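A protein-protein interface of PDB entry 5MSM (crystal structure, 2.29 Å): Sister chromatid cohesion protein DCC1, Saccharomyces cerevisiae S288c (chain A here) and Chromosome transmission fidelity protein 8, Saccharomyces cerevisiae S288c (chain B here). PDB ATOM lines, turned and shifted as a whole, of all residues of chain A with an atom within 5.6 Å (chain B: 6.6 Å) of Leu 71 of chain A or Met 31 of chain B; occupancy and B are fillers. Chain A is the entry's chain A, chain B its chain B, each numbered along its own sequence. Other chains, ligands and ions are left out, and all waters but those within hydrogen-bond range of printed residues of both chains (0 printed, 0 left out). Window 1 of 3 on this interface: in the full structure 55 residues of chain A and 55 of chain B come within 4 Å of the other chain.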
ATOM      1  N   ILE A   3       8.081  -7.377 -25.682  1.00  0.00           N
ATOM      2  CA  ILE A   3       8.007  -6.611 -24.454  1.00  0.00           C
ATOM      3  C   ILE A   3       8.428  -7.461 -23.265  1.00  0.00           C
ATOM      4  O   ILE A   3       7.832  -8.524 -23.051  1.00  0.00           O
ATOM      5  CB  ILE A   3       6.568  -6.106 -24.252  1.00  0.00           C
ATOM      6  CG1 ILE A   3       6.137  -5.338 -25.514  1.00  0.00           C
ATOM      7  CG2 ILE A   3       6.438  -5.294 -22.962  1.00  0.00           C
ATOM      8  CD1 ILE A   3       4.733  -4.869 -25.501  1.00  0.00           C
ATOM      9  N   LEU A   5       8.405  -8.568 -19.467  1.00  0.00           N
ATOM     10  CA  LEU A   5       7.368  -8.558 -18.453  1.00  0.00           C
ATOM     11  C   LEU A   5       7.945  -8.768 -17.064  1.00  0.00           C
ATOM     12  O   LEU A   5       8.616  -9.780 -16.807  1.00  0.00           O
ATOM     13  CB  LEU A   5       6.324  -9.636 -18.738  1.00  0.00           C
ATOM     14  CG  LEU A   5       5.751  -9.694 -20.151  1.00  0.00           C
ATOM     15  CD1 LEU A   5       4.875 -10.899 -20.250  1.00  0.00           C
ATOM     16  CD2 LEU A   5       4.972  -8.456 -20.521  1.00  0.00           C
ATOM     17  N   TYR A  15      -5.880  -0.510  -6.331  1.00  0.00           N
ATOM     18  CA  TYR A  15      -6.266  -0.442  -7.744  1.00  0.00           C
ATOM     19  C   TYR A  15      -7.355  -1.459  -8.073  1.00  0.00           C
ATOM     20  O   TYR A  15      -7.151  -2.650  -7.871  1.00  0.00           O
ATOM     21  CB  TYR A  15      -5.061  -0.702  -8.680  1.00  0.00           C
ATOM     22  CG  TYR A  15      -3.969   0.314  -8.581  1.00  0.00           C
ATOM     23  CD1 TYR A  15      -4.052   1.522  -9.242  1.00  0.00           C
ATOM     24  CD2 TYR A  15      -2.870   0.081  -7.788  1.00  0.00           C
ATOM     25  CE1 TYR A  15      -3.030   2.456  -9.136  1.00  0.00           C
ATOM     26  CE2 TYR A  15      -1.853   1.003  -7.671  1.00  0.00           C
ATOM     27  CZ  TYR A  15      -1.930   2.180  -8.347  1.00  0.00           C
ATOM     28  OH  TYR A  15      -0.906   3.085  -8.214  1.00  0.00           O
ATOM     29  N   LEU A  17     -10.862  -2.508 -10.925  1.00  0.00           N
ATOM     30  CA  LEU A  17     -11.455  -2.331 -12.256  1.00  0.00           C
ATOM     31  C   LEU A  17     -12.955  -2.101 -12.192  1.00  0.00           C
ATOM     32  O   LEU A  17     -13.684  -2.896 -11.603  1.00  0.00           O
ATOM     33  CB  LEU A  17     -11.191  -3.553 -13.156  1.00  0.00           C
ATOM     34  CG  LEU A  17      -9.771  -3.880 -13.617  1.00  0.00           C
ATOM     35  CD1 LEU A  17      -9.688  -5.251 -14.291  1.00  0.00           C
ATOM     36  CD2 LEU A  17      -9.328  -2.816 -14.588  1.00  0.00           C
ATOM     37  N   VAL A  69      -5.363 -11.735 -13.682  1.00  0.00           N
ATOM     38  CA  VAL A  69      -5.352 -10.492 -14.443  1.00  0.00           C
ATOM     39  C   VAL A  69      -4.330  -9.568 -13.825  1.00  0.00           C
ATOM     40  O   VAL A  69      -4.469  -9.158 -12.665  1.00  0.00           O
ATOM     41  CB  VAL A  69      -6.700  -9.809 -14.494  1.00  0.00           C
ATOM     42  CG1 VAL A  69      -6.577  -8.468 -15.255  1.00  0.00           C
ATOM     43  CG2 VAL A  69      -7.702 -10.709 -15.168  1.00  0.00           C
ATOM     44  N   LEU A  70      -3.278  -9.286 -14.588  1.00  0.00           N
ATOM     45  CA  LEU A  70      -2.278  -8.319 -14.190  1.00  0.00           C
ATOM     46  C   LEU A  70      -2.464  -7.021 -14.931  1.00  0.00           C
ATOM     47  O   LEU A  70      -2.636  -7.014 -16.157  1.00  0.00           O
ATOM     48  CB  LEU A  70      -0.874  -8.831 -14.457  1.00  0.00           C
ATOM     49  CG  LEU A  70      -0.446 -10.018 -13.612  1.00  0.00           C
ATOM     50  CD1 LEU A  70       0.958 -10.419 -14.061  1.00  0.00           C
ATOM     51  CD2 LEU A  70      -0.506  -9.676 -12.127  1.00  0.00           C
ATOM     52  N   LEU A  71      -2.446  -5.930 -14.173  1.00  0.00           N
ATOM     53  CA  LEU A  71      -2.402  -4.588 -14.733  1.00  0.00           C
ATOM     54  C   LEU A  71      -0.924  -4.246 -14.800  1.00  0.00           C
ATOM     55  O   LEU A  71      -0.190  -4.419 -13.814  1.00  0.00           O
ATOM     56  CB  LEU A  71      -3.195  -3.611 -13.869  1.00  0.00           C
ATOM     57  CG  LEU A  71      -4.615  -4.150 -13.661  1.00  0.00           C
ATOM     58  CD1 LEU A  71      -5.512  -3.155 -12.954  1.00  0.00           C
ATOM     59  CD2 LEU A  71      -5.200  -4.501 -15.000  1.00  0.00           C
ATOM     60  N   MET A  72      -0.465  -3.840 -15.976  1.00  0.00           N
ATOM     61  CA  MET A  72       0.957  -3.617 -16.152  1.00  0.00           C
ATOM     62  C   MET A  72       1.153  -2.199 -16.657  1.00  0.00           C
ATOM     63  O   MET A  72       0.295  -1.684 -17.374  1.00  0.00           O
ATOM     64  CB  MET A  72       1.544  -4.662 -17.107  1.00  0.00           C
ATOM     65  CG  MET A  72       1.099  -6.080 -16.758  1.00  0.00           C
ATOM     66  SD  MET A  72       2.026  -7.428 -17.519  1.00  0.00           S
ATOM     67  CE  MET A  72       3.529  -7.342 -16.552  1.00  0.00           C
ATOM     68  N   ARG A  73       2.254  -1.563 -16.250  1.00  0.00           N
ATOM     69  CA  ARG A  73       2.601  -0.225 -16.726  1.00  0.00           C
ATOM     70  C   ARG A  73       4.018  -0.204 -17.273  1.00  0.00           C
ATOM     71  O   ARG A  73       4.910  -0.876 -16.775  1.00  0.00           O
ATOM     72  CB  ARG A  73       2.498   0.825 -15.622  1.00  0.00           C
ATOM     73  CG  ARG A  73       3.443   0.584 -14.459  1.00  0.00           C
ATOM     74  CD  ARG A  73       3.370   1.693 -13.431  1.00  0.00           C
ATOM     75  NE  ARG A  73       4.475   1.615 -12.466  1.00  0.00           N
ATOM     76  CZ  ARG A  73       5.725   2.042 -12.698  1.00  0.00           C
ATOM     77  NH1 ARG A  73       6.072   2.550 -13.879  1.00  0.00           N
ATOM     78  NH2 ARG A  73       6.647   1.940 -11.754  1.00  0.00           N
ATOM     79  N   VAL A  98       7.515  -3.639 -19.148  1.00  0.00           N
ATOM     80  CA  VAL A  98       6.332  -3.314 -18.339  1.00  0.00           C
ATOM     81  C   VAL A  98       6.347  -4.094 -17.041  1.00  0.00           C
ATOM     82  O   VAL A  98       6.910  -5.203 -16.984  1.00  0.00           O
ATOM     83  CB  VAL A  98       4.995  -3.595 -19.079  1.00  0.00           C
ATOM     84  CG1 VAL A  98       4.845  -2.709 -20.306  1.00  0.00           C
ATOM     85  CG2 VAL A  98       4.864  -5.047 -19.435  1.00  0.00           C
ATOM     86  N   VAL A  99       5.756  -3.504 -15.997  1.00  0.00           N
ATOM     87  CA  VAL A  99       5.654  -4.134 -14.669  1.00  0.00           C
ATOM     88  C   VAL A  99       4.207  -4.311 -14.158  1.00  0.00           C
ATOM     89  O   VAL A  99       3.389  -3.408 -14.241  1.00  0.00           O
ATOM     90  CB  VAL A  99       6.478  -3.332 -13.604  1.00  0.00           C
ATOM     91  CG1 VAL A  99       6.084  -1.884 -13.545  1.00  0.00           C
ATOM     92  CG2 VAL A  99       6.389  -3.988 -12.243  1.00  0.00           C
ATOM     93  N   GLY A 100       3.891  -5.500 -13.659  1.00  0.00           N
ATOM     94  CA  GLY A 100       2.585  -5.740 -13.078  1.00  0.00           C
ATOM     95  C   GLY A 100       2.506  -5.071 -11.727  1.00  0.00           C
ATOM     96  O   GLY A 100       3.199  -5.507 -10.799  1.00  0.00           O
ATOM     97  N   PHE A 101       1.681  -4.026 -11.609  1.00  0.00           N
ATOM     98  CA  PHE A 101       1.522  -3.330 -10.325  1.00  0.00           C
ATOM     99  C   PHE A 101       0.271  -3.750  -9.556  1.00  0.00           C
ATOM    100  O   PHE A 101       0.189  -3.539  -8.346  1.00  0.00           O
ATOM    101  CB  PHE A 101       1.507  -1.806 -10.517  1.00  0.00           C
ATOM    102  CG  PHE A 101       0.359  -1.287 -11.352  1.00  0.00           C
ATOM    103  CD1 PHE A 101       0.424  -1.315 -12.733  1.00  0.00           C
ATOM    104  CD2 PHE A 101      -0.748  -0.711 -10.751  1.00  0.00           C
ATOM    105  CE1 PHE A 101      -0.605  -0.822 -13.497  1.00  0.00           C
ATOM    106  CE2 PHE A 101      -1.793  -0.197 -11.508  1.00  0.00           C
ATOM    107  CZ  PHE A 101      -1.729  -0.251 -12.875  1.00  0.00           C
ATOM    108  N   ALA A 102      -0.719  -4.299 -10.251  1.00  0.00           N
ATOM    109  CA  ALA A 102      -1.909  -4.827  -9.572  1.00  0.00           C
ATOM    110  C   ALA A 102      -2.369  -6.121 -10.221  1.00  0.00           C
ATOM    111  O   ALA A 102      -2.221  -6.322 -11.436  1.00  0.00           O
ATOM    112  CB  ALA A 102      -3.046  -3.807  -9.568  1.00  0.00           C
ATOM    113  N   LYS A 103      -2.929  -6.984  -9.390  1.00  0.00           N
ATOM    114  CA  LYS A 103      -3.479  -8.253  -9.806  1.00  0.00           C
ATOM    115  C   LYS A 103      -4.905  -8.355  -9.308  1.00  0.00           C
ATOM    116  O   LYS A 103      -5.123  -8.456  -8.099  1.00  0.00           O
ATOM    117  CB  LYS A 103      -2.657  -9.389  -9.247  1.00  0.00           C
ATOM    118  CG  LYS A 103      -3.199 -10.779  -9.534  1.00  0.00           C
ATOM    119  CD  LYS A 103      -2.246 -11.816  -8.942  1.00  0.00           C
ATOM    120  CE  LYS A 103      -2.830 -13.192  -9.048  1.00  0.00           C
ATOM    121  NZ  LYS A 103      -4.157 -13.275  -8.347  1.00  0.00           N
ATOM    122  N   THR A 104      -5.874  -8.342 -10.221  1.00  0.00           N
ATOM    123  CA  THR A 104      -7.282  -8.290  -9.832  1.00  0.00           C
ATOM    124  C   THR A 104      -7.949  -9.646 -10.063  1.00  0.00           C
ATOM    125  O   THR A 104      -7.739 -10.269 -11.109  1.00  0.00           O
ATOM    126  CB  THR A 104      -8.015  -7.212 -10.639  1.00  0.00           C
ATOM    127  OG1 THR A 104      -7.973  -7.563 -12.032  1.00  0.00           O
ATOM    128  CG2 THR A 104      -7.337  -5.874 -10.446  1.00  0.00           C
ATOM    129  N   THR B  23      -4.040  -1.593 -30.824  1.00  0.00           N
ATOM    130  CA  THR B  23      -3.739  -1.350 -29.418  1.00  0.00           C
ATOM    131  C   THR B  23      -2.378  -0.820 -28.963  1.00  0.00           C
ATOM    132  O   THR B  23      -2.272   0.345 -28.573  1.00  0.00           O
ATOM    133  CB  THR B  23      -3.974  -2.660 -28.639  1.00  0.00           C
ATOM    134  OG1 THR B  23      -3.363  -2.564 -27.342  1.00  0.00           O
ATOM    135  CG2 THR B  23      -3.355  -3.838 -29.386  1.00  0.00           C
ATOM    136  N   VAL B  24      -1.359  -1.678 -29.010  1.00  0.00           N
ATOM    137  CA  VAL B  24      -0.053  -1.433 -28.407  1.00  0.00           C
ATOM    138  C   VAL B  24      -0.307  -1.373 -26.876  1.00  0.00           C
ATOM    139  O   VAL B  24      -0.818  -2.326 -26.270  1.00  0.00           O
ATOM    140  CB  VAL B  24       0.676  -0.135 -28.921  1.00  0.00           C
ATOM    141  CG1 VAL B  24       2.167  -0.185 -28.601  1.00  0.00           C
ATOM    142  CG2 VAL B  24       0.515   0.039 -30.410  1.00  0.00           C
ATOM    143  N   ILE B  25       0.027  -0.242 -26.269  1.00  0.00           N
ATOM    144  CA  ILE B  25      -0.225   0.035 -24.872  1.00  0.00           C
ATOM    145  C   ILE B  25      -1.210   1.216 -24.828  1.00  0.00           C
ATOM    146  O   ILE B  25      -1.394   1.858 -25.866  1.00  0.00           O
ATOM    147  CB  ILE B  25       1.108   0.348 -24.173  1.00  0.00           C
ATOM    148  CG1 ILE B  25       2.087  -0.819 -24.348  1.00  0.00           C
ATOM    149  CG2 ILE B  25       0.911   0.662 -22.745  1.00  0.00           C
ATOM    150  CD1 ILE B  25       1.653  -2.134 -23.744  1.00  0.00           C
ATOM    151  N   THR B  26      -1.898   1.490 -23.710  1.00  0.00           N
ATOM    152  CA  THR B  26      -2.667   2.752 -23.659  1.00  0.00           C
ATOM    153  C   THR B  26      -1.671   3.885 -23.779  1.00  0.00           C
ATOM    154  O   THR B  26      -0.505   3.709 -23.428  1.00  0.00           O
ATOM    155  CB  THR B  26      -3.469   3.000 -22.352  1.00  0.00           C
ATOM    156  OG1 THR B  26      -2.568   3.295 -21.274  1.00  0.00           O
ATOM    157  CG2 THR B  26      -4.379   1.833 -22.007  1.00  0.00           C
ATOM    158  N   GLY B  29       0.518   4.408 -20.958  1.00  0.00           N
ATOM    159  CA  GLY B  29       1.538   3.415 -20.698  1.00  0.00           C
ATOM    160  C   GLY B  29       1.072   2.180 -19.947  1.00  0.00           C
ATOM    161  O   GLY B  29       1.875   1.510 -19.298  1.00  0.00           O
ATOM    162  N   MET B  30      -0.215   1.863 -20.009  1.00  0.00           N
ATOM    163  CA  MET B  30      -0.714   0.706 -19.271  1.00  0.00           C
ATOM    164  C   MET B  30      -1.341  -0.357 -20.165  1.00  0.00           C
ATOM    165  O   MET B  30      -1.760  -0.075 -21.296  1.00  0.00           O
ATOM    166  CB  MET B  30      -1.708   1.167 -18.206  1.00  0.00           C
ATOM    167  CG  MET B  30      -0.992   1.607 -16.923  1.00  0.00           C
ATOM    168  SD  MET B  30      -1.959   2.612 -15.791  1.00  0.00           S
ATOM    169  CE  MET B  30      -1.865   4.249 -16.571  1.00  0.00           C
ATOM    170  N   MET B  31      -1.385  -1.583 -19.661  1.00  0.00           N
ATOM    171  CA  MET B  31      -1.983  -2.680 -20.404  1.00  0.00           C
ATOM    172  C   MET B  31      -2.561  -3.718 -19.463  1.00  0.00           C
ATOM    173  O   MET B  31      -2.253  -3.732 -18.275  1.00  0.00           O
ATOM    174  CB  MET B  31      -0.959  -3.350 -21.323  1.00  0.00           C
ATOM    175  CG  MET B  31       0.191  -3.970 -20.574  1.00  0.00           C
ATOM    176  SD  MET B  31       1.193  -5.090 -21.612  1.00  0.00           S
ATOM    177  CE  MET B  31       0.098  -6.505 -21.642  1.00  0.00           C
ATOM    178  N   MET B  32      -3.401  -4.590 -20.004  1.00  0.00           N
ATOM    179  CA  MET B  32      -4.073  -5.590 -19.207  1.00  0.00           C
ATOM    180  C   MET B  32      -3.722  -6.975 -19.723  1.00  0.00           C
ATOM    181  O   MET B  32      -3.980  -7.299 -20.874  1.00  0.00           O
ATOM    182  CB  MET B  32      -5.583  -5.355 -19.239  1.00  0.00           C
ATOM    183  CG  MET B  32      -6.414  -6.325 -18.446  1.00  0.00           C
ATOM    184  SD  MET B  32      -8.166  -5.890 -18.583  1.00  0.00           S
ATOM    185  CE  MET B  32      -8.902  -7.535 -18.549  1.00  0.00           C
ATOM    186  N   LEU B  33      -3.121  -7.787 -18.865  1.00  0.00           N
ATOM    187  CA  LEU B  33      -2.702  -9.123 -19.244  1.00  0.00           C
ATOM    188  C   LEU B  33      -3.556 -10.191 -18.561  1.00  0.00           C
ATOM    189  O   LEU B  33      -3.666 -10.205 -17.330  1.00  0.00           O
ATOM    190  CB  LEU B  33      -1.231  -9.315 -18.874  1.00  0.00           C
ATOM    191  CG  LEU B  33      -0.720 -10.743 -18.948  1.00  0.00           C
ATOM    192  CD1 LEU B  33      -0.819 -11.207 -20.410  1.00  0.00           C
ATOM    193  CD2 LEU B  33       0.709 -10.816 -18.425  1.00  0.00           C
ATOM    194  N   LEU B  73       6.457 -10.825 -24.099  1.00  0.00           N
ATOM    195  CA  LEU B  73       5.227 -10.820 -24.864  1.00  0.00           C
ATOM    196  C   LEU B  73       5.499 -10.354 -26.294  1.00  0.00           C
ATOM    197  O   LEU B  73       6.073  -9.279 -26.503  1.00  0.00           O
ATOM    198  CB  LEU B  73       4.202  -9.909 -24.196  1.00  0.00           C
ATOM    199  CG  LEU B  73       2.885  -9.591 -24.908  1.00  0.00           C
ATOM    200  CD1 LEU B  73       2.074 -10.835 -25.068  1.00  0.00           C
ATOM    201  CD2 LEU B  73       2.132  -8.563 -24.090  1.00  0.00           C
ATOM    202  N   ILE B 103      -9.554   1.837 -14.598  1.00  0.00           N
ATOM    203  CA  ILE B 103      -8.688   1.490 -13.505  1.00  0.00           C
ATOM    204  C   ILE B 103      -8.829   2.646 -12.536  1.00  0.00           C
ATOM    205  O   ILE B 103      -8.470   3.784 -12.855  1.00  0.00           O
ATOM    206  CB  ILE B 103      -7.234   1.324 -13.928  1.00  0.00           C
ATOM    207  CG1 ILE B 103      -7.085   0.188 -14.947  1.00  0.00           C
ATOM    208  CG2 ILE B 103      -6.384   1.062 -12.714  1.00  0.00           C
ATOM    209  CD1 ILE B 103      -5.680   0.100 -15.552  1.00  0.00           C
ATOM    210  N   ASP B 117      -6.597   5.100 -15.472  1.00  0.00           N
ATOM    211  CA  ASP B 117      -6.556   4.877 -16.906  1.00  0.00           C
ATOM    212  C   ASP B 117      -7.814   4.161 -17.321  1.00  0.00           C
ATOM    213  O   ASP B 117      -8.585   3.696 -16.475  1.00  0.00           O
ATOM    214  CB  ASP B 117      -5.359   4.042 -17.311  1.00  0.00           C
ATOM    215  CG  ASP B 117      -4.876   4.357 -18.727  1.00  0.00           C
ATOM    216  OD1 ASP B 117      -5.631   4.963 -19.525  1.00  0.00           O
ATOM    217  OD2 ASP B 117      -3.731   3.961 -19.036  1.00  0.00           O
ATOM    218  N   MET B 119      -9.058   1.011 -19.795  1.00  0.00           N
ATOM    219  CA  MET B 119      -8.585  -0.128 -20.565  1.00  0.00           C
ATOM    220  C   MET B 119      -9.615  -0.458 -21.616  1.00  0.00           C
ATOM    221  O   MET B 119     -10.788  -0.642 -21.282  1.00  0.00           O
ATOM    222  CB  MET B 119      -8.364  -1.353 -19.682  1.00  0.00           C
ATOM    223  CG  MET B 119      -7.276  -1.209 -18.618  1.00  0.00           C
ATOM    224  SD  MET B 119      -5.631  -0.864 -19.274  1.00  0.00           S
ATOM    225  CE  MET B 119      -5.631  -1.985 -20.671  1.00  0.00           C
ATOM    226  N   TYR B 121      -8.487  -2.582 -24.436  1.00  0.00           N
ATOM    227  CA  TYR B 121      -7.994  -3.823 -24.999  1.00  0.00           C
ATOM    228  C   TYR B 121      -7.335  -4.607 -23.905  1.00  0.00           C
ATOM    229  O   TYR B 121      -6.872  -4.036 -22.918  1.00  0.00           O
ATOM    230  CB  TYR B 121      -7.001  -3.554 -26.129  1.00  0.00           C
ATOM    231  CG  TYR B 121      -7.655  -2.922 -27.318  1.00  0.00           C
ATOM    232  CD1 TYR B 121      -7.809  -1.550 -27.398  1.00  0.00           C
ATOM    233  CD2 TYR B 121      -8.149  -3.703 -28.351  1.00  0.00           C
ATOM    234  CE1 TYR B 121      -8.418  -0.969 -28.481  1.00  0.00           C
ATOM    235  CE2 TYR B 121      -8.757  -3.128 -29.443  1.00  0.00           C
ATOM    236  CZ  TYR B 121      -8.896  -1.762 -29.500  1.00  0.00           C
ATOM    237  OH  TYR B 121      -9.512  -1.200 -30.592  1.00  0.00           O
ATOM    238  N   LYS B 122      -7.275  -5.916 -24.088  1.00  0.00           N
ATOM    239  CA  LYS B 122      -6.526  -6.780 -23.197  1.00  0.00           C
ATOM    240  C   LYS B 122      -5.816  -7.797 -24.054  1.00  0.00           C
ATOM    241  O   LYS B 122      -6.171  -7.974 -25.213  1.00  0.00           O
ATOM    242  CB  LYS B 122      -7.451  -7.455 -22.178  1.00  0.00           C
ATOM    243  CG  LYS B 122      -8.398  -8.477 -22.785  1.00  0.00           C
ATOM    244  CD  LYS B 122      -9.138  -9.235 -21.715  1.00  0.00           C
ATOM    245  CE  LYS B 122     -10.214 -10.139 -22.274  1.00  0.00           C
ATOM    246  NZ  LYS B 122     -10.868 -10.845 -21.120  1.00  0.00           N
ATOM    247  N   VAL B 123      -4.805  -8.462 -23.509  1.00  0.00           N
ATOM    248  CA  VAL B 123      -4.183  -9.582 -24.214  1.00  0.00           C
ATOM    249  C   VAL B 123      -4.381 -10.787 -23.315  1.00  0.00           C
ATOM    250  O   VAL B 123      -4.047 -10.760 -22.134  1.00  0.00           O
ATOM    251  CB  VAL B 123      -2.703  -9.329 -24.553  1.00  0.00           C
ATOM    252  CG1 VAL B 123      -1.896  -8.981 -23.301  1.00  0.00           C
ATOM    253  CG2 VAL B 123      -2.103 -10.546 -25.279  1.00  0.00           C
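Of the 16 printed residues of chain A, 7 touch a printed residue of chain B.
Hydrophobic or aromatic side chains of chain A within 4 Å of the printed part of chain B: Ile 3, Leu 17, Val 69 and Met 72.
Of the 16 printed residues of chain B, 7 touch a printed residue of chain A.
Hydrophobic or aromatic side chains of chain B within 4 Å of the printed part of chain A: Met 30, Met 31, Met 32, Leu 33 and Ile 103.
Among the printed residues, 13 pairs touch across the chains.
Among the printed residues, no Asp or Glu carboxylate lies within 4 Å of a Lys or Arg side-chain nitrogen of the other chain.
Leu 71 of chain A touches one residue of chain B.
Of the printed residues of chain A, Met 31 of chain B touches Leu 70 (3.9 Å), Leu 71 (3.6 Å) and Met 72 (2.8 Å).
Of the printed residues of chain A, Leu 33 of chain B touches Val 69, Leu 70 and Met 72.
Printed residues of chain A within 4 Å of Met 32 of chain B: Val 69 (3.8 Å) and Leu 70 (3.7 Å).
Of the printed residues of chain B, Leu 70 of chain A touches Met 31, Met 32 and Leu 33.
Met 119 of chain B touches none of the printed residues of chain A.
Phe 101 of chain A touches none of the printed residues of chain B.
The nearest residue of chain B that does not touch Leu 71 of chain A is Met 32 of chain B (4.1 Å).
The nearest residue of chain A that does not touch Met 31 of chain B is Val 98 of chain A (4.3 Å).
The nearest printed residue of chain A that does not touch Ile 103 of chain B is Leu 71 of chain A (4.2 Å).
Among the printed residues, pairs that only touch across the chains: Leu 17 of chain A with Ile 103 of chain B, Val 69 of chain A with Met 32 of chain B, Val 69 of chain A with Leu 33 of chain B, Leu 70 of chain A with Met 31 of chain B, Leu 70 of chain A with Met 32 of chain B, Leu 71 of chain A with Met 31 of chain B, Met 72 of chain A with Met 30 of chain B, Met 72 of chain A with Leu 33 of chain B, Arg 73 of chain A with Gly 29 of chain B and Arg 73 of chain A with Met 30 of chain B.
The backbone carbonyl oxygen (O) of Ala 102 of chain A sits at hydrogen-bond distance from the backbone NH (N) of Leu 71 of chain A.
The backbone NH (N) of Thr 104 of chain A sits at hydrogen-bond distance from the backbone carbonyl oxygen (O) of Val 69 of chain A (2.9 Å).
N of Ile 103 of chain B lies within hydrogen-bond range of O of Asp 117 of chain B (2.8 Å).
N of Val 123 of chain B is in hydrogen-bond range of O of Met 32 of chain B (3.0 Å).
O of Leu 71 of chain A sits at hydrogen-bond distance from N of Phe 101 of chain A (2.9 Å).
OG1 of Thr 26 of chain B sits at hydrogen-bond distance from N of Gly 29 of chain B (3.3 Å).
The backbone NH (N) of Leu 33 of chain B lies within hydrogen-bond range of the backbone carbonyl oxygen (O) of Leu 70 of chain A.
The backbone NH (N) of Leu 73 of chain B sits at hydrogen-bond distance from the backbone carbonyl oxygen (O) of Ile 3 of chain A (2.9 Å).
N of Met 31 of chain B lies within hydrogen-bond range of O of Met 72 of chain A, at 2.8 Å.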
